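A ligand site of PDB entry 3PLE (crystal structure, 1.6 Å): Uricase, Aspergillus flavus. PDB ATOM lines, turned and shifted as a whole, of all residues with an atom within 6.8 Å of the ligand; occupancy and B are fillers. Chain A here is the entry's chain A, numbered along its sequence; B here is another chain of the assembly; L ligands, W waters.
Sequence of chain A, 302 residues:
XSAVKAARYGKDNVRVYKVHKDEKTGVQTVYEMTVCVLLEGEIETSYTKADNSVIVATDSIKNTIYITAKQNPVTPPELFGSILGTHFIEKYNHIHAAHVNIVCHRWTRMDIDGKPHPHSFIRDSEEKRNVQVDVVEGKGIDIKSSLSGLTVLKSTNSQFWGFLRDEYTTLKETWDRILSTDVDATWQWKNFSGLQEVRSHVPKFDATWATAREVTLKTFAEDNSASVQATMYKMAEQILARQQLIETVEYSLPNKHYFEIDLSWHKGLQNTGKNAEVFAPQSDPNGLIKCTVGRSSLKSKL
Water W1 bridges N5 of the ligand (2.7 Å) and NH1 of Arg 177 (3.4 Å).
The backbone NH (N) of Thr 58 of chain B is in hydrogen-bond range of a nitrogen (N3) of the ligand (2.8 Å).
OG1 of Thr 58 of chain B is in hydrogen-bond range of N3 of the ligand (3.2 Å).
NH2 of Arg 177 is in hydrogen-bond range of O1 of the ligand (2.8 Å).
The side-chain amide nitrogen (NE2) of Gln 229 sits at hydrogen-bond distance from an oxygen (O2) of the ligand (2.9 Å).
N of Val 228 sits at hydrogen-bond distance from O1 of the ligand.
A nitrogen (N2) of the ligand lies close to the side-chain amide nitrogen (ND2) of Asn 255.
The side-chain amino group of Lys 11 of chain B sits at hydrogen-bond distance from the side-chain hydroxyl of Thr 58 of chain B.
The backbone NH (N) of Arg 177 lies within hydrogen-bond range of the backbone carbonyl oxygen (O) of Ser 158, 2.9 Å away.
N of Gln 229 lies close to OG of Ser 227 (3.4 Å).
The backbone carbonyl oxygen of Asn 255 is in hydrogen-bond range of a ring nitrogen (NE2) of His 257.
The backbone NH (N) of Asn 255 sits at hydrogen-bond distance from the backbone carbonyl oxygen (O) of Gly 287.
OG of Ser 225 is in hydrogen-bond range of O of Ser 227.
The side-chain hydroxyl (OH) of Tyr 9 of chain B is in hydrogen-bond range of the backbone carbonyl oxygen (O) of Val 56 of chain B.
Phe 160 touches the ligand (CE2 to C2, 3.4 Å).
CD2 of Leu 171 touches N4 of the ligand, at 3.8 Å.
CA of Ser 227 touches O1 of the ligand, 3.6 Å away.
CD2 of Tyr 9 of chain B touches O2 of the ligand (3.8 Å).
Ile 55 of chain B touches the ligand.
CA of Ala 57 of chain B touches N3 of the ligand, at 3.5 Å.
Asp 59 of chain B touches the ligand (N to N4, 3.9 Å).
Hydrophobic or aromatic side chains that line the ligand: Phe 160, Leu 171, Val 228, Tyr 9 of chain B, Ile 55 of chain B and Ala 57 of chain B.
12 residues have an atom within 4 Å of the ligand: Phe 160, Leu 171, Arg 177, Ser 227, Val 228, Gln 229, Asn 255, Tyr 9 of chain B, Ile 55 of chain B, Ala 57 of chain B, Thr 58 of chain B and Asp 59 of chain B.
Along chain A the residues within 4 Å of the ligand span positions 160 to 255.
The nearest printed residue that does not touch the ligand is Ile 289 (4.1 Å).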
ATOM      1  N   SER A 158       8.050  -0.786  11.788  1.00  0.00           N
ATOM      2  CA  SER A 158       8.758   0.188  12.600  1.00  0.00           C
ATOM      3  C   SER A 158      10.192   0.205  12.072  1.00  0.00           C
ATOM      4  O   SER A 158      10.785  -0.849  11.803  1.00  0.00           O
ATOM      5  CB  SER A 158       8.731  -0.195  14.093  1.00  0.00           C
ATOM      6  OG  SER A 158       9.634   0.610  14.834  1.00  0.00           O
ATOM      7  N   GLN A 159      10.730   1.416  11.925  1.00  0.00           N
ATOM      8  CA  GLN A 159      12.069   1.639  11.404  1.00  0.00           C
ATOM      9  C   GLN A 159      12.805   2.600  12.319  1.00  0.00           C
ATOM     10  O   GLN A 159      12.194   3.373  13.074  1.00  0.00           O
ATOM     11  CB  GLN A 159      11.981   2.284  10.002  1.00  0.00           C
ATOM     12  CG  GLN A 159      11.137   1.496   9.014  1.00  0.00           C
ATOM     13  CD  GLN A 159      11.112   2.099   7.613  1.00  0.00           C
ATOM     14  OE1 GLN A 159      11.830   3.055   7.308  1.00  0.00           O
ATOM     15  NE2 GLN A 159      10.286   1.527   6.760  1.00  0.00           N
ATOM     16  N   PHE A 160      14.120   2.558  12.260  1.00  0.00           N
ATOM     17  CA  PHE A 160      14.922   3.565  12.916  1.00  0.00           C
ATOM     18  C   PHE A 160      16.288   3.685  12.269  1.00  0.00           C
ATOM     19  O   PHE A 160      17.195   2.894  12.516  1.00  0.00           O
ATOM     20  CB  PHE A 160      15.011   3.319  14.458  1.00  0.00           C
ATOM     21  CG  PHE A 160      15.576   4.507  15.196  1.00  0.00           C
ATOM     22  CD1 PHE A 160      14.889   5.721  15.194  1.00  0.00           C
ATOM     23  CD2 PHE A 160      16.807   4.438  15.852  1.00  0.00           C
ATOM     24  CE1 PHE A 160      15.412   6.832  15.831  1.00  0.00           C
ATOM     25  CE2 PHE A 160      17.322   5.543  16.511  1.00  0.00           C
ATOM     26  CZ  PHE A 160      16.635   6.762  16.479  1.00  0.00           C
ATOM     27  N   PHE A 163      19.854   8.395  12.303  1.00  0.00           N
ATOM     28  CA  PHE A 163      20.235   9.102  13.525  1.00  0.00           C
ATOM     29  C   PHE A 163      21.715   9.505  13.534  1.00  0.00           C
ATOM     30  O   PHE A 163      22.489   9.021  12.716  1.00  0.00           O
ATOM     31  CB  PHE A 163      19.909   8.268  14.771  1.00  0.00           C
ATOM     32  CG  PHE A 163      20.393   6.840  14.680  1.00  0.00           C
ATOM     33  CD1 PHE A 163      19.591   5.871  14.119  1.00  0.00           C
ATOM     34  CD2 PHE A 163      21.655   6.487  15.162  1.00  0.00           C
ATOM     35  CE1 PHE A 163      20.007   4.555  14.023  1.00  0.00           C
ATOM     36  CE2 PHE A 163      22.085   5.171  15.067  1.00  0.00           C
ATOM     37  CZ  PHE A 163      21.276   4.220  14.494  1.00  0.00           C
ATOM     38  N   LEU A 171      24.845   1.419  17.607  1.00  0.00           N
ATOM     39  CA  LEU A 171      23.544   0.970  17.112  1.00  0.00           C
ATOM     40  C   LEU A 171      23.506   0.924  15.591  1.00  0.00           C
ATOM     41  O   LEU A 171      23.880   1.898  14.931  1.00  0.00           O
ATOM     42  CB  LEU A 171      22.451   1.924  17.611  1.00  0.00           C
ATOM     43  CG  LEU A 171      21.003   1.558  17.223  1.00  0.00           C
ATOM     44  CD1 LEU A 171      20.558   0.291  17.940  1.00  0.00           C
ATOM     45  CD2 LEU A 171      20.057   2.696  17.577  1.00  0.00           C
ATOM     46  N   ARG A 177      11.888  -3.407  12.612  1.00  0.00           N
ATOM     47  CA  ARG A 177      12.115  -3.824  13.997  1.00  0.00           C
ATOM     48  C   ARG A 177      10.790  -3.995  14.709  1.00  0.00           C
ATOM     49  O   ARG A 177       9.743  -3.565  14.230  1.00  0.00           O
ATOM     50  CB  ARG A 177      12.974  -2.795  14.735  1.00  0.00           C
ATOM     51  CG  ARG A 177      12.274  -1.457  14.927  1.00  0.00           C
ATOM     52  CD  ARG A 177      13.133  -0.457  15.670  1.00  0.00           C
ATOM     53  NE  ARG A 177      12.345   0.757  15.954  1.00  0.00           N
ATOM     54  CZ  ARG A 177      12.729   1.754  16.732  1.00  0.00           C
ATOM     55  NH1 ARG A 177      13.912   1.746  17.327  1.00  0.00           N
ATOM     56  NH2 ARG A 177      11.917   2.808  16.907  1.00  0.00           N
ATOM     57  N   LEU A 179       8.364  -2.900  17.747  1.00  0.00           N
ATOM     58  CA  LEU A 179       8.137  -1.718  18.570  1.00  0.00           C
ATOM     59  C   LEU A 179       7.109  -2.069  19.637  1.00  0.00           C
ATOM     60  O   LEU A 179       6.012  -2.513  19.321  1.00  0.00           O
ATOM     61  CB  LEU A 179       7.661  -0.546  17.707  1.00  0.00           C
ATOM     62  CG  LEU A 179       7.388   0.772  18.428  1.00  0.00           C
ATOM     63  CD1 LEU A 179       8.647   1.290  19.083  1.00  0.00           C
ATOM     64  CD2 LEU A 179       6.840   1.811  17.429  1.00  0.00           C
ATOM     65  N   SER A 225       6.298   3.482  11.223  1.00  0.00           N
ATOM     66  CA  SER A 225       6.891   4.392  12.174  1.00  0.00           C
ATOM     67  C   SER A 225       8.364   4.694  11.892  1.00  0.00           C
ATOM     68  O   SER A 225       9.186   3.791  11.770  1.00  0.00           O
ATOM     69  CB  SER A 225       6.739   3.804  13.580  1.00  0.00           C
ATOM     70  OG  SER A 225       7.449   4.574  14.505  1.00  0.00           O
ATOM     71  N   ALA A 226       8.698   5.983  11.823  1.00  0.00           N
ATOM     72  CA  ALA A 226      10.061   6.415  11.575  1.00  0.00           C
ATOM     73  C   ALA A 226      10.865   6.475  12.867  1.00  0.00           C
ATOM     74  O   ALA A 226      12.097   6.524  12.849  1.00  0.00           O
ATOM     75  CB  ALA A 226      10.048   7.795  10.916  1.00  0.00           C
ATOM     76  N   SER A 227      10.135   6.512  13.991  1.00  0.00           N
ATOM     77  CA  SER A 227      10.728   6.613  15.318  1.00  0.00           C
ATOM     78  C   SER A 227       9.569   6.697  16.296  1.00  0.00           C
ATOM     79  O   SER A 227       8.440   6.970  15.893  1.00  0.00           O
ATOM     80  CB  SER A 227      11.576   7.879  15.478  1.00  0.00           C
ATOM     81  OG  SER A 227      10.762   9.051  15.396  1.00  0.00           O
ATOM     82  N   VAL A 228       9.830   6.496  17.587  1.00  0.00           N
ATOM     83  CA  VAL A 228       8.780   6.679  18.570  1.00  0.00           C
ATOM     84  C   VAL A 228       8.332   8.139  18.562  1.00  0.00           C
ATOM     85  O   VAL A 228       7.136   8.432  18.622  1.00  0.00           O
ATOM     86  CB  VAL A 228       9.290   6.257  19.971  1.00  0.00           C
ATOM     87  CG1 VAL A 228       8.284   6.606  21.041  1.00  0.00           C
ATOM     88  CG2 VAL A 228       9.574   4.747  19.966  1.00  0.00           C
ATOM     89  N   GLN A 229       9.308   9.043  18.462  1.00  0.00           N
ATOM     90  CA  GLN A 229       9.080  10.490  18.407  1.00  0.00           C
ATOM     91  C   GLN A 229       8.035  10.840  17.338  1.00  0.00           C
ATOM     92  O   GLN A 229       7.052  11.558  17.605  1.00  0.00           O
ATOM     93  CB  GLN A 229      10.400  11.208  18.103  1.00  0.00           C
ATOM     94  CG  GLN A 229      11.389  11.254  19.282  1.00  0.00           C
ATOM     95  CD  GLN A 229      12.323  10.058  19.362  1.00  0.00           C
ATOM     96  OE1 GLN A 229      12.012   8.951  18.897  1.00  0.00           O
ATOM     97  NE2 GLN A 229      13.476  10.278  19.982  1.00  0.00           N
ATOM     98  N   ASN A 255      10.559   2.693  25.300  1.00  0.00           N
ATOM     99  CA  ASN A 255      10.826   1.880  24.142  1.00  0.00           C
ATOM    100  C   ASN A 255      11.336   0.556  24.722  1.00  0.00           C
ATOM    101  O   ASN A 255      12.463   0.501  25.210  1.00  0.00           O
ATOM    102  CB  ASN A 255      11.819   2.615  23.238  1.00  0.00           C
ATOM    103  CG  ASN A 255      12.006   1.944  21.897  1.00  0.00           C
ATOM    104  OD1 ASN A 255      11.329   0.980  21.565  1.00  0.00           O
ATOM    105  ND2 ASN A 255      12.943   2.467  21.109  1.00  0.00           N
ATOM    106  N   HIS A 257      12.747  -2.816  24.487  1.00  0.00           N
ATOM    107  CA  HIS A 257      13.548  -3.414  23.417  1.00  0.00           C
ATOM    108  C   HIS A 257      13.437  -4.927  23.338  1.00  0.00           C
ATOM    109  O   HIS A 257      13.427  -5.617  24.346  1.00  0.00           O
ATOM    110  CB  HIS A 257      15.013  -3.017  23.570  1.00  0.00           C
ATOM    111  CG  HIS A 257      15.215  -1.540  23.691  1.00  0.00           C
ATOM    112  ND1 HIS A 257      14.975  -0.667  22.651  1.00  0.00           N
ATOM    113  CD2 HIS A 257      15.613  -0.773  24.731  1.00  0.00           C
ATOM    114  CE1 HIS A 257      15.240   0.571  23.043  1.00  0.00           C
ATOM    115  NE2 HIS A 257      15.618   0.534  24.306  1.00  0.00           N
ATOM    116  N   GLY A 287      14.578   2.826  26.406  1.00  0.00           N
ATOM    117  CA  GLY A 287      14.415   4.217  25.966  1.00  0.00           C
ATOM    118  C   GLY A 287      13.207   4.819  26.647  1.00  0.00           C
ATOM    119  O   GLY A 287      12.289   4.112  27.073  1.00  0.00           O
ATOM    120  N   ILE A 289      10.787   8.300  25.955  1.00  0.00           N
ATOM    121  CA  ILE A 289      10.579   9.381  25.009  1.00  0.00           C
ATOM    122  C   ILE A 289       9.348  10.145  25.447  1.00  0.00           C
ATOM    123  O   ILE A 289       8.306   9.529  25.670  1.00  0.00           O
ATOM    124  CB  ILE A 289      10.337   8.828  23.582  1.00  0.00           C
ATOM    125  CG1 ILE A 289      11.355   7.725  23.208  1.00  0.00           C
ATOM    126  CG2 ILE A 289      10.350   9.985  22.573  1.00  0.00           C
ATOM    127  CD1 ILE A 289      12.763   8.099  23.279  1.00  0.00           C
ATOM    128  N   TYR B   9      14.025  13.189  25.921  1.00  0.00           N
ATOM    129  CA  TYR B   9      14.101  11.767  25.627  1.00  0.00           C
ATOM    130  C   TYR B   9      15.465  11.255  26.086  1.00  0.00           C
ATOM    131  O   TYR B   9      16.415  12.020  26.246  1.00  0.00           O
ATOM    132  CB  TYR B   9      13.881  11.514  24.119  1.00  0.00           C
ATOM    133  CG  TYR B   9      15.158  11.708  23.353  1.00  0.00           C
ATOM    134  CD1 TYR B   9      15.676  12.981  23.158  1.00  0.00           C
ATOM    135  CD2 TYR B   9      15.886  10.620  22.911  1.00  0.00           C
ATOM    136  CE1 TYR B   9      16.909  13.155  22.509  1.00  0.00           C
ATOM    137  CE2 TYR B   9      17.105  10.782  22.249  1.00  0.00           C
ATOM    138  CZ  TYR B   9      17.609  12.058  22.069  1.00  0.00           C
ATOM    139  OH  TYR B   9      18.820  12.236  21.441  1.00  0.00           O
ATOM    140  N   GLY B  10      15.561   9.949  26.295  1.00  0.00           N
ATOM    141  CA  GLY B  10      16.847   9.398  26.696  1.00  0.00           C
ATOM    142  C   GLY B  10      16.719   7.947  27.095  1.00  0.00           C
ATOM    143  O   GLY B  10      15.886   7.227  26.569  1.00  0.00           O
ATOM    144  N   LYS B  11      17.558   7.540  28.036  1.00  0.00           N
ATOM    145  CA  LYS B  11      17.607   6.118  28.452  1.00  0.00           C
ATOM    146  C   LYS B  11      17.325   6.054  29.939  1.00  0.00           C
ATOM    147  O   LYS B  11      17.909   6.823  30.721  1.00  0.00           O
ATOM    148  CB  LYS B  11      18.982   5.510  28.174  1.00  0.00           C
ATOM    149  CG  LYS B  11      18.998   3.987  28.055  1.00  0.00           C
ATOM    150  CD  LYS B  11      18.141   3.521  26.876  1.00  0.00           C
ATOM    151  CE  LYS B  11      18.817   2.479  26.038  1.00  0.00           C
ATOM    152  NZ  LYS B  11      18.066   2.278  24.757  1.00  0.00           N
ATOM    153  N   ASN B  52      15.552  12.241  11.878  1.00  0.00           N
ATOM    154  CA  ASN B  52      16.349  11.568  12.915  1.00  0.00           C
ATOM    155  C   ASN B  52      17.760  12.118  13.070  1.00  0.00           C
ATOM    156  O   ASN B  52      18.494  11.718  13.974  1.00  0.00           O
ATOM    157  CB  ASN B  52      16.330  10.052  12.715  1.00  0.00           C
ATOM    158  CG  ASN B  52      14.970   9.441  12.986  1.00  0.00           C
ATOM    159  OD1 ASN B  52      14.164  10.023  13.722  1.00  0.00           O
ATOM    160  ND2 ASN B  52      14.701   8.275  12.417  1.00  0.00           N
ATOM    161  N   ILE B  55      18.870  13.272  16.471  1.00  0.00           N
ATOM    162  CA  ILE B  55      18.754  12.331  17.593  1.00  0.00           C
ATOM    163  C   ILE B  55      20.080  11.644  17.917  1.00  0.00           C
ATOM    164  O   ILE B  55      20.622  10.910  17.084  1.00  0.00           O
ATOM    165  CB  ILE B  55      17.699  11.238  17.346  1.00  0.00           C
ATOM    166  CG1 ILE B  55      16.285  11.827  17.210  1.00  0.00           C
ATOM    167  CG2 ILE B  55      17.709  10.216  18.554  1.00  0.00           C
ATOM    168  CD1 ILE B  55      15.218  10.785  16.782  1.00  0.00           C
ATOM    169  N   VAL B  56      20.571  11.899  19.124  1.00  0.00           N
ATOM    170  CA  VAL B  56      21.609  11.084  19.727  1.00  0.00           C
ATOM    171  C   VAL B  56      20.863   9.842  20.188  1.00  0.00           C
ATOM    172  O   VAL B  56      19.995   9.943  21.071  1.00  0.00           O
ATOM    173  CB  VAL B  56      22.275  11.847  20.898  1.00  0.00           C
ATOM    174  CG1 VAL B  56      23.296  10.973  21.625  1.00  0.00           C
ATOM    175  CG2 VAL B  56      22.931  13.143  20.377  1.00  0.00           C
ATOM    176  N   ALA B  57      21.138   8.679  19.599  1.00  0.00           N
ATOM    177  CA  ALA B  57      20.317   7.487  19.871  1.00  0.00           C
ATOM    178  C   ALA B  57      20.361   7.154  21.370  1.00  0.00           C
ATOM    179  O   ALA B  57      21.393   7.339  22.003  1.00  0.00           O
ATOM    180  CB  ALA B  57      20.763   6.275  19.019  1.00  0.00           C
ATOM    181  N   THR B  58      19.242   6.674  21.907  1.00  0.00           N
ATOM    182  CA  THR B  58      19.230   6.340  23.334  1.00  0.00           C
ATOM    183  C   THR B  58      20.272   5.257  23.617  1.00  0.00           C
ATOM    184  O   THR B  58      20.885   5.254  24.696  1.00  0.00           O
ATOM    185  CB  THR B  58      17.838   5.929  23.822  1.00  0.00           C
ATOM    186  OG1 THR B  58      17.468   4.688  23.222  1.00  0.00           O
ATOM    187  CG2 THR B  58      16.804   7.023  23.487  1.00  0.00           C
ATOM    188  N   ASP B  59      20.485   4.356  22.653  1.00  0.00           N
ATOM    189  CA  ASP B  59      21.536   3.332  22.804  1.00  0.00           C
ATOM    190  C   ASP B  59      22.907   3.962  23.003  1.00  0.00           C
ATOM    191  O   ASP B  59      23.717   3.468  23.787  1.00  0.00           O
ATOM    192  CB  ASP B  59      21.553   2.412  21.584  1.00  0.00           C
ATOM    193  CG  ASP B  59      22.444   1.209  21.794  1.00  0.00           C
ATOM    194  OD1 ASP B  59      22.007   0.262  22.485  1.00  0.00           O
ATOM    195  OD2 ASP B  59      23.559   1.208  21.232  1.00  0.00           O
ATOM    196  N   SER B  60      23.178   5.071  22.284  1.00  0.00           N
ATOM    197  CA  SER B  60      24.445   5.810  22.457  1.00  0.00           C
ATOM    198  C   SER B  60      24.556   6.486  23.812  1.00  0.00           C
ATOM    199  O   SER B  60      25.636   6.610  24.391  1.00  0.00           O
ATOM    200  CB  SER B  60      24.605   6.840  21.320  1.00  0.00           C
ATOM    201  OG  SER B  60      24.444   6.166  20.086  1.00  0.00           O
HETATM  202  N1  LIG L   1      13.832   6.642  19.121  1.00  0.00           N
HETATM  203  C1  LIG L   1      13.518   5.414  18.663  1.00  0.00           C
HETATM  204  O1  LIG L   1      12.379   5.247  18.177  1.00  0.00           O
HETATM  205  N2  LIG L   1      14.356   4.338  18.721  1.00  0.00           N
HETATM  206  C2  LIG L   1      15.601   4.516  19.227  1.00  0.00           C
HETATM  207  C3  LIG L   1      16.009   5.842  19.733  1.00  0.00           C
HETATM  208  C4  LIG L   1      15.030   6.945  19.641  1.00  0.00           C
HETATM  209  O2  LIG L   1      15.314   8.080  20.086  1.00  0.00           O
HETATM  210  N3  LIG L   1      17.269   5.755  20.176  1.00  0.00           N
HETATM  211  N4  LIG L   1      17.672   4.436  19.995  1.00  0.00           N
HETATM  212  N5  LIG L   1      16.656   3.699  19.400  1.00  0.00           N
HETATM  213  O   HOH W   1      16.645   0.973  19.185  1.00  0.00           O
